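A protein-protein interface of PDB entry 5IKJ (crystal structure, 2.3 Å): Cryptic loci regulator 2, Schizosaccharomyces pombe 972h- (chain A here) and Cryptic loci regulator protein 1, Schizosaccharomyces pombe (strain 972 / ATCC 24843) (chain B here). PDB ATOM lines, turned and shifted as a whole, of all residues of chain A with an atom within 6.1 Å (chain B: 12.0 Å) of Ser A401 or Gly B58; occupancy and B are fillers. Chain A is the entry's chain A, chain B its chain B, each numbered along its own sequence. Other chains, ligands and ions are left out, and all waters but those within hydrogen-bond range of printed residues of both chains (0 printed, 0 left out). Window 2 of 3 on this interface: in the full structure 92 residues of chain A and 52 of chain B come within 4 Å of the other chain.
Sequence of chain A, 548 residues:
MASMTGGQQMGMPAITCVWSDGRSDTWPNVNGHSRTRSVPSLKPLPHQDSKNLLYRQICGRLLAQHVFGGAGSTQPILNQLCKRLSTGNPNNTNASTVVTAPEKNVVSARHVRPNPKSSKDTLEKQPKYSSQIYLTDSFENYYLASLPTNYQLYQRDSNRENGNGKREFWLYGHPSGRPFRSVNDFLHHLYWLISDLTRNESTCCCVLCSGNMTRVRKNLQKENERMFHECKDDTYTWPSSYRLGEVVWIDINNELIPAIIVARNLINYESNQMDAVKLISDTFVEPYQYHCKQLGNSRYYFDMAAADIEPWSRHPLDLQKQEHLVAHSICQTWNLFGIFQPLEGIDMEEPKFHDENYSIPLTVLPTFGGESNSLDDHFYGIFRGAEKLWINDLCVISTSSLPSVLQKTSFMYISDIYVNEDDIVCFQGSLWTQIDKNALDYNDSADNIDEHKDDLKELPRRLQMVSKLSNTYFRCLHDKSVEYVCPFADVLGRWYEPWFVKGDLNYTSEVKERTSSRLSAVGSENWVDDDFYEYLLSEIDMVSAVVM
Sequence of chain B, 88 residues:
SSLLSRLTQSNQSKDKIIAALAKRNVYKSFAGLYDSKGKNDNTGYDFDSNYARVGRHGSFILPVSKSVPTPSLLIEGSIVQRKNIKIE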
ATOM      1  N   SER A 398       1.370  25.789  21.947  1.00  0.00           N
ATOM      2  CA  SER A 398       1.425  27.238  21.804  1.00  0.00           C
ATOM      3  C   SER A 398       0.588  27.903  22.888  1.00  0.00           C
ATOM      4  O   SER A 398      -0.562  27.521  23.122  1.00  0.00           O
ATOM      5  CB  SER A 398       0.915  27.654  20.425  1.00  0.00           C
ATOM      6  OG  SER A 398       1.668  27.041  19.393  1.00  0.00           O
ATOM      7  N   THR A 399       1.171  28.898  23.550  1.00  0.00           N
ATOM      8  CA  THR A 399       0.460  29.698  24.538  1.00  0.00           C
ATOM      9  C   THR A 399       0.006  31.042  23.988  1.00  0.00           C
ATOM     10  O   THR A 399      -0.627  31.813  24.716  1.00  0.00           O
ATOM     11  CB  THR A 399       1.341  29.929  25.772  1.00  0.00           C
ATOM     12  OG1 THR A 399       2.589  30.510  25.370  1.00  0.00           O
ATOM     13  CG2 THR A 399       1.600  28.619  26.501  1.00  0.00           C
ATOM     14  N   SER A 400       0.310  31.340  22.724  1.00  0.00           N
ATOM     15  CA  SER A 400      -0.027  32.627  22.129  1.00  0.00           C
ATOM     16  C   SER A 400      -1.516  32.922  22.257  1.00  0.00           C
ATOM     17  O   SER A 400      -1.915  33.813  23.015  1.00  0.00           O
ATOM     18  CB  SER A 400       0.393  32.653  20.659  1.00  0.00           C
ATOM     19  OG  SER A 400      -0.196  31.581  19.943  1.00  0.00           O
ATOM     20  N   SER A 401      -2.345  32.183  21.522  1.00  0.00           N
ATOM     21  CA  SER A 401      -3.795  32.374  21.552  1.00  0.00           C
ATOM     22  C   SER A 401      -4.346  31.536  22.698  1.00  0.00           C
ATOM     23  O   SER A 401      -4.664  30.356  22.541  1.00  0.00           O
ATOM     24  CB  SER A 401      -4.416  31.993  20.215  1.00  0.00           C
ATOM     25  OG  SER A 401      -3.764  32.661  19.147  1.00  0.00           O
ATOM     26  N   LEU A 402      -4.464  32.159  23.868  1.00  0.00           N
ATOM     27  CA  LEU A 402      -4.793  31.444  25.094  1.00  0.00           C
ATOM     28  C   LEU A 402      -5.000  32.461  26.214  1.00  0.00           C
ATOM     29  O   LEU A 402      -4.162  33.353  26.394  1.00  0.00           O
ATOM     30  CB  LEU A 402      -3.671  30.455  25.423  1.00  0.00           C
ATOM     31  CG  LEU A 402      -3.590  29.765  26.785  1.00  0.00           C
ATOM     32  CD1 LEU A 402      -4.495  28.543  26.873  1.00  0.00           C
ATOM     33  CD2 LEU A 402      -2.152  29.351  27.039  1.00  0.00           C
ATOM     34  N   PRO A 403      -6.102  32.374  26.984  1.00  0.00           N
ATOM     35  CA  PRO A 403      -6.398  33.425  27.970  1.00  0.00           C
ATOM     36  C   PRO A 403      -5.245  33.730  28.916  1.00  0.00           C
ATOM     37  O   PRO A 403      -4.344  32.907  29.106  1.00  0.00           O
ATOM     38  CB  PRO A 403      -7.610  32.867  28.734  1.00  0.00           C
ATOM     39  CG  PRO A 403      -7.663  31.410  28.393  1.00  0.00           C
ATOM     40  CD  PRO A 403      -7.119  31.311  27.009  1.00  0.00           C
ATOM     41  N   GLN A 407      -1.486  31.337  30.472  1.00  0.00           N
ATOM     42  CA  GLN A 407      -0.242  31.551  29.742  1.00  0.00           C
ATOM     43  C   GLN A 407       0.984  31.047  30.492  1.00  0.00           C
ATOM     44  O   GLN A 407       2.060  30.957  29.891  1.00  0.00           O
ATOM     45  CB  GLN A 407      -0.077  33.033  29.408  1.00  0.00           C
ATOM     46  CG  GLN A 407      -1.319  33.642  28.784  1.00  0.00           C
ATOM     47  CD  GLN A 407      -1.024  34.463  27.546  1.00  0.00           C
ATOM     48  OE1 GLN A 407      -1.126  33.970  26.421  1.00  0.00           O
ATOM     49  NE2 GLN A 407      -0.668  35.726  27.743  1.00  0.00           N
ATOM     50  N   ALA A 489      -2.331  21.471  15.246  1.00  0.00           N
ATOM     51  CA  ALA A 489      -1.562  22.616  14.769  1.00  0.00           C
ATOM     52  C   ALA A 489      -0.895  23.379  15.907  1.00  0.00           C
ATOM     53  O   ALA A 489       0.134  24.029  15.693  1.00  0.00           O
ATOM     54  CB  ALA A 489      -2.471  23.557  13.978  1.00  0.00           C
ATOM     55  N   ASP A 490      -1.458  23.325  17.113  1.00  0.00           N
ATOM     56  CA  ASP A 490      -0.933  24.073  18.248  1.00  0.00           C
ATOM     57  C   ASP A 490      -0.078  23.222  19.177  1.00  0.00           C
ATOM     58  O   ASP A 490       0.365  23.720  20.217  1.00  0.00           O
ATOM     59  CB  ASP A 490      -2.084  24.710  19.039  1.00  0.00           C
ATOM     60  CG  ASP A 490      -2.714  25.881  18.307  1.00  0.00           C
ATOM     61  OD1 ASP A 490      -1.989  26.588  17.578  1.00  0.00           O
ATOM     62  OD2 ASP A 490      -3.934  26.095  18.460  1.00  0.00           O
ATOM     63  N   VAL B  54      -4.202  18.709  10.033  1.00  0.00           N
ATOM     64  CA  VAL B  54      -3.565  19.416  11.140  1.00  0.00           C
ATOM     65  C   VAL B  54      -4.407  20.449  11.873  1.00  0.00           C
ATOM     66  O   VAL B  54      -4.332  20.547  13.089  1.00  0.00           O
ATOM     67  CB  VAL B  54      -2.260  20.075  10.654  1.00  0.00           C
ATOM     68  CG1 VAL B  54      -1.599  20.891  11.748  1.00  0.00           C
ATOM     69  CG2 VAL B  54      -1.314  19.001  10.160  1.00  0.00           C
ATOM     70  N   GLY B  55      -5.188  21.229  11.151  1.00  0.00           N
ATOM     71  CA  GLY B  55      -5.993  22.241  11.793  1.00  0.00           C
ATOM     72  C   GLY B  55      -5.418  23.621  11.569  1.00  0.00           C
ATOM     73  O   GLY B  55      -4.548  23.807  10.727  1.00  0.00           O
ATOM     74  N   ARG B  56      -5.909  24.593  12.324  1.00  0.00           N
ATOM     75  CA  ARG B  56      -5.465  25.972  12.167  1.00  0.00           C
ATOM     76  C   ARG B  56      -4.615  26.398  13.356  1.00  0.00           C
ATOM     77  O   ARG B  56      -5.042  26.281  14.509  1.00  0.00           O
ATOM     78  CB  ARG B  56      -6.657  26.919  12.015  1.00  0.00           C
ATOM     79  CG  ARG B  56      -6.241  28.368  11.815  1.00  0.00           C
ATOM     80  CD  ARG B  56      -7.372  29.239  11.281  1.00  0.00           C
ATOM     81  NE  ARG B  56      -8.004  28.687  10.084  1.00  0.00           N
ATOM     82  CZ  ARG B  56      -7.407  28.567   8.902  1.00  0.00           C
ATOM     83  NH1 ARG B  56      -6.144  28.941   8.740  1.00  0.00           N
ATOM     84  NH2 ARG B  56      -8.074  28.060   7.876  1.00  0.00           N
ATOM     85  N   HIS B  57      -3.418  26.900  13.062  1.00  0.00           N
ATOM     86  CA  HIS B  57      -2.536  27.421  14.095  1.00  0.00           C
ATOM     87  C   HIS B  57      -3.149  28.657  14.745  1.00  0.00           C
ATOM     88  O   HIS B  57      -3.944  29.379  14.136  1.00  0.00           O
ATOM     89  CB  HIS B  57      -1.174  27.771  13.488  1.00  0.00           C
ATOM     90  CG  HIS B  57      -0.043  27.746  14.469  1.00  0.00           C
ATOM     91  ND1 HIS B  57       0.159  28.742  15.400  1.00  0.00           N
ATOM     92  CD2 HIS B  57       0.960  26.853  14.650  1.00  0.00           C
ATOM     93  CE1 HIS B  57       1.231  28.458  16.119  1.00  0.00           C
ATOM     94  NE2 HIS B  57       1.735  27.318  15.685  1.00  0.00           N
ATOM     95  N   GLY B  58      -2.778  28.893  16.001  1.00  0.00           N
ATOM     96  CA  GLY B  58      -3.190  30.101  16.692  1.00  0.00           C
ATOM     97  C   GLY B  58      -4.682  30.254  16.879  1.00  0.00           C
ATOM     98  O   GLY B  58      -5.155  31.370  17.113  1.00  0.00           O
ATOM     99  N   SER B  59      -5.443  29.170  16.784  1.00  0.00           N
ATOM    100  CA  SER B  59      -6.882  29.227  17.005  1.00  0.00           C
ATOM    101  C   SER B  59      -7.151  29.363  18.504  1.00  0.00           C
ATOM    102  O   SER B  59      -6.238  29.505  19.321  1.00  0.00           O
ATOM    103  CB  SER B  59      -7.557  27.996  16.409  1.00  0.00           C
ATOM    104  OG  SER B  59      -6.982  26.803  16.915  1.00  0.00           O
ATOM    105  N   PHE B  60      -8.426  29.322  18.882  1.00  0.00           N
ATOM    106  CA  PHE B  60      -8.805  29.373  20.284  1.00  0.00           C
ATOM    107  C   PHE B  60      -8.777  27.976  20.890  1.00  0.00           C
ATOM    108  O   PHE B  60      -9.056  26.977  20.221  1.00  0.00           O
ATOM    109  CB  PHE B  60     -10.195  29.990  20.460  1.00  0.00           C
ATOM    110  CG  PHE B  60     -10.196  31.495  20.459  1.00  0.00           C
ATOM    111  CD1 PHE B  60      -9.532  32.202  21.449  1.00  0.00           C
ATOM    112  CD2 PHE B  60     -10.870  32.201  19.477  1.00  0.00           C
ATOM    113  CE1 PHE B  60      -9.533  33.583  21.455  1.00  0.00           C
ATOM    114  CE2 PHE B  60     -10.875  33.584  19.478  1.00  0.00           C
ATOM    115  CZ  PHE B  60     -10.206  34.275  20.469  1.00  0.00           C
ATOM    116  N   ILE B  61      -8.440  27.921  22.174  1.00  0.00           N
ATOM    117  CA  ILE B  61      -8.305  26.676  22.919  1.00  0.00           C
ATOM    118  C   ILE B  61      -9.420  26.664  23.957  1.00  0.00           C
ATOM    119  O   ILE B  61      -9.427  27.479  24.887  1.00  0.00           O
ATOM    120  CB  ILE B  61      -6.916  26.545  23.563  1.00  0.00           C
ATOM    121  CG1 ILE B  61      -6.869  25.357  24.530  1.00  0.00           C
ATOM    122  CG2 ILE B  61      -6.516  27.844  24.260  1.00  0.00           C
ATOM    123  CD1 ILE B  61      -5.480  25.057  25.062  1.00  0.00           C
ATOM    124  N   LEU B  62     -10.364  25.738  23.800  1.00  0.00           N
ATOM    125  CA  LEU B  62     -11.636  25.839  24.493  1.00  0.00           C
ATOM    126  C   LEU B  62     -11.764  24.787  25.592  1.00  0.00           C
ATOM    127  O   LEU B  62     -11.254  23.670  25.456  1.00  0.00           O
ATOM    128  CB  LEU B  62     -12.793  25.673  23.503  1.00  0.00           C
ATOM    129  CG  LEU B  62     -12.678  26.539  22.246  1.00  0.00           C
ATOM    130  CD1 LEU B  62     -13.718  26.134  21.216  1.00  0.00           C
ATOM    131  CD2 LEU B  62     -12.805  28.013  22.598  1.00  0.00           C
ATOM    132  N   PRO B  63     -12.442  25.109  26.691  1.00  0.00           N
ATOM    133  CA  PRO B  63     -12.666  24.111  27.741  1.00  0.00           C
ATOM    134  C   PRO B  63     -13.769  23.131  27.378  1.00  0.00           C
ATOM    135  O   PRO B  63     -14.705  23.450  26.643  1.00  0.00           O
ATOM    136  CB  PRO B  63     -13.071  24.963  28.950  1.00  0.00           C
ATOM    137  CG  PRO B  63     -13.714  26.164  28.346  1.00  0.00           C
ATOM    138  CD  PRO B  63     -12.948  26.437  27.082  1.00  0.00           C
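The side-chain hydroxyl (OG) of Ser B59 is in hydrogen-bond range of the side-chain carboxylate (OD2) of Asp A490 (3.5 Å).
OD1 of Asp A490 is in hydrogen-bond range of N of Gly B58, at 2.9 Å.
The side-chain hydroxyl of Ser A401 is in hydrogen-bond range of the backbone carbonyl oxygen of Gly B58, at 2.8 Å.
N of Ala A489 sits at hydrogen-bond distance from O of Val B54, at 3.1 Å.
Ser A401 touches just these residues of chain B: Gly B58, Ser B59 and Ile B61.
Of the printed residues of chain A, Gly B58 touches Ser A401 (2.8 Å) and Asp A490 (2.9 Å).
Of chain B, only His B57 (3.6 Å) comes within 4 Å of Ser A398.
No residue of chain B comes within 4 Å of Thr A399.
No residue of chain B comes within 4 Å of Ser A400.
Printed residues of chain B within 4 Å of Leu A402: Ile B61.
Pro A403 touches none of the printed residues of chain B.
Ala A489 touches just these residues of chain B: Val B54 (3.1 Å), Gly B55 (3.8 Å), Arg B56 (3.6 Å) and His B57 (3.1 Å).
Of chain B, only His B57, Gly B58 and Ser B59 come within 4 Å of Asp A490.
Printed residues of chain A within 4 Å of Arg B56: Ala A489.
Of the printed residues of chain A, Ile B61 touches Ser A401 and Leu A402.
Printed residues of chain A within 4 Å of Val B54: Ala A489.
Of the printed residues of chain A, Ser B59 touches Ser A401 and Asp A490.
The nearest residue of chain A that does not touch Gly B58 is Ser A400 (4.7 Å).
The nearest printed residue of chain A that does not touch Arg B56 is Asp A490 (4.1 Å).
The backbone carbonyl oxygen of Arg B56 is in hydrogen-bond range of the side-chain hydroxyl of Ser B59 (3.1 Å).
The backbone carbonyl oxygen of Asp A490 is in hydrogen-bond range of the backbone NH of Ser A398, 2.9 Å away.
O of Leu A402 sits close to OE1 of Gln A407 (3.1 Å).
Ser A398 touches His B57 (OG to CE1, 3.6 Å).
Ser A401 touches Ser B59.
Ser A401 touches Ile B61 (O to CG2, 3.6 Å).
Leu A402 touches Ile B61 (CD1 to CG2, 3.4 Å).
Gly B55 touches Ala A489 (C to CB, 3.8 Å).
Ala A489 touches Arg B56 (CB to C, 3.6 Å).
His B57 touches Ala A489 (CD2 to O, 3.1 Å).
Asp A490 touches His B57 (OD1 to CA, 3.6 Å).
Of the 9 printed residues of chain A, 5 touch a printed residue of chain B.
Printed residues of chain A that touch a printed residue of chain B: Ser A398, Ser A401, Leu A402, Ala A489 and Asp A490.
Among the printed residues, no Asp or Glu carboxylate lies within 4 Å of a Lys or Arg side-chain nitrogen of the other chain.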
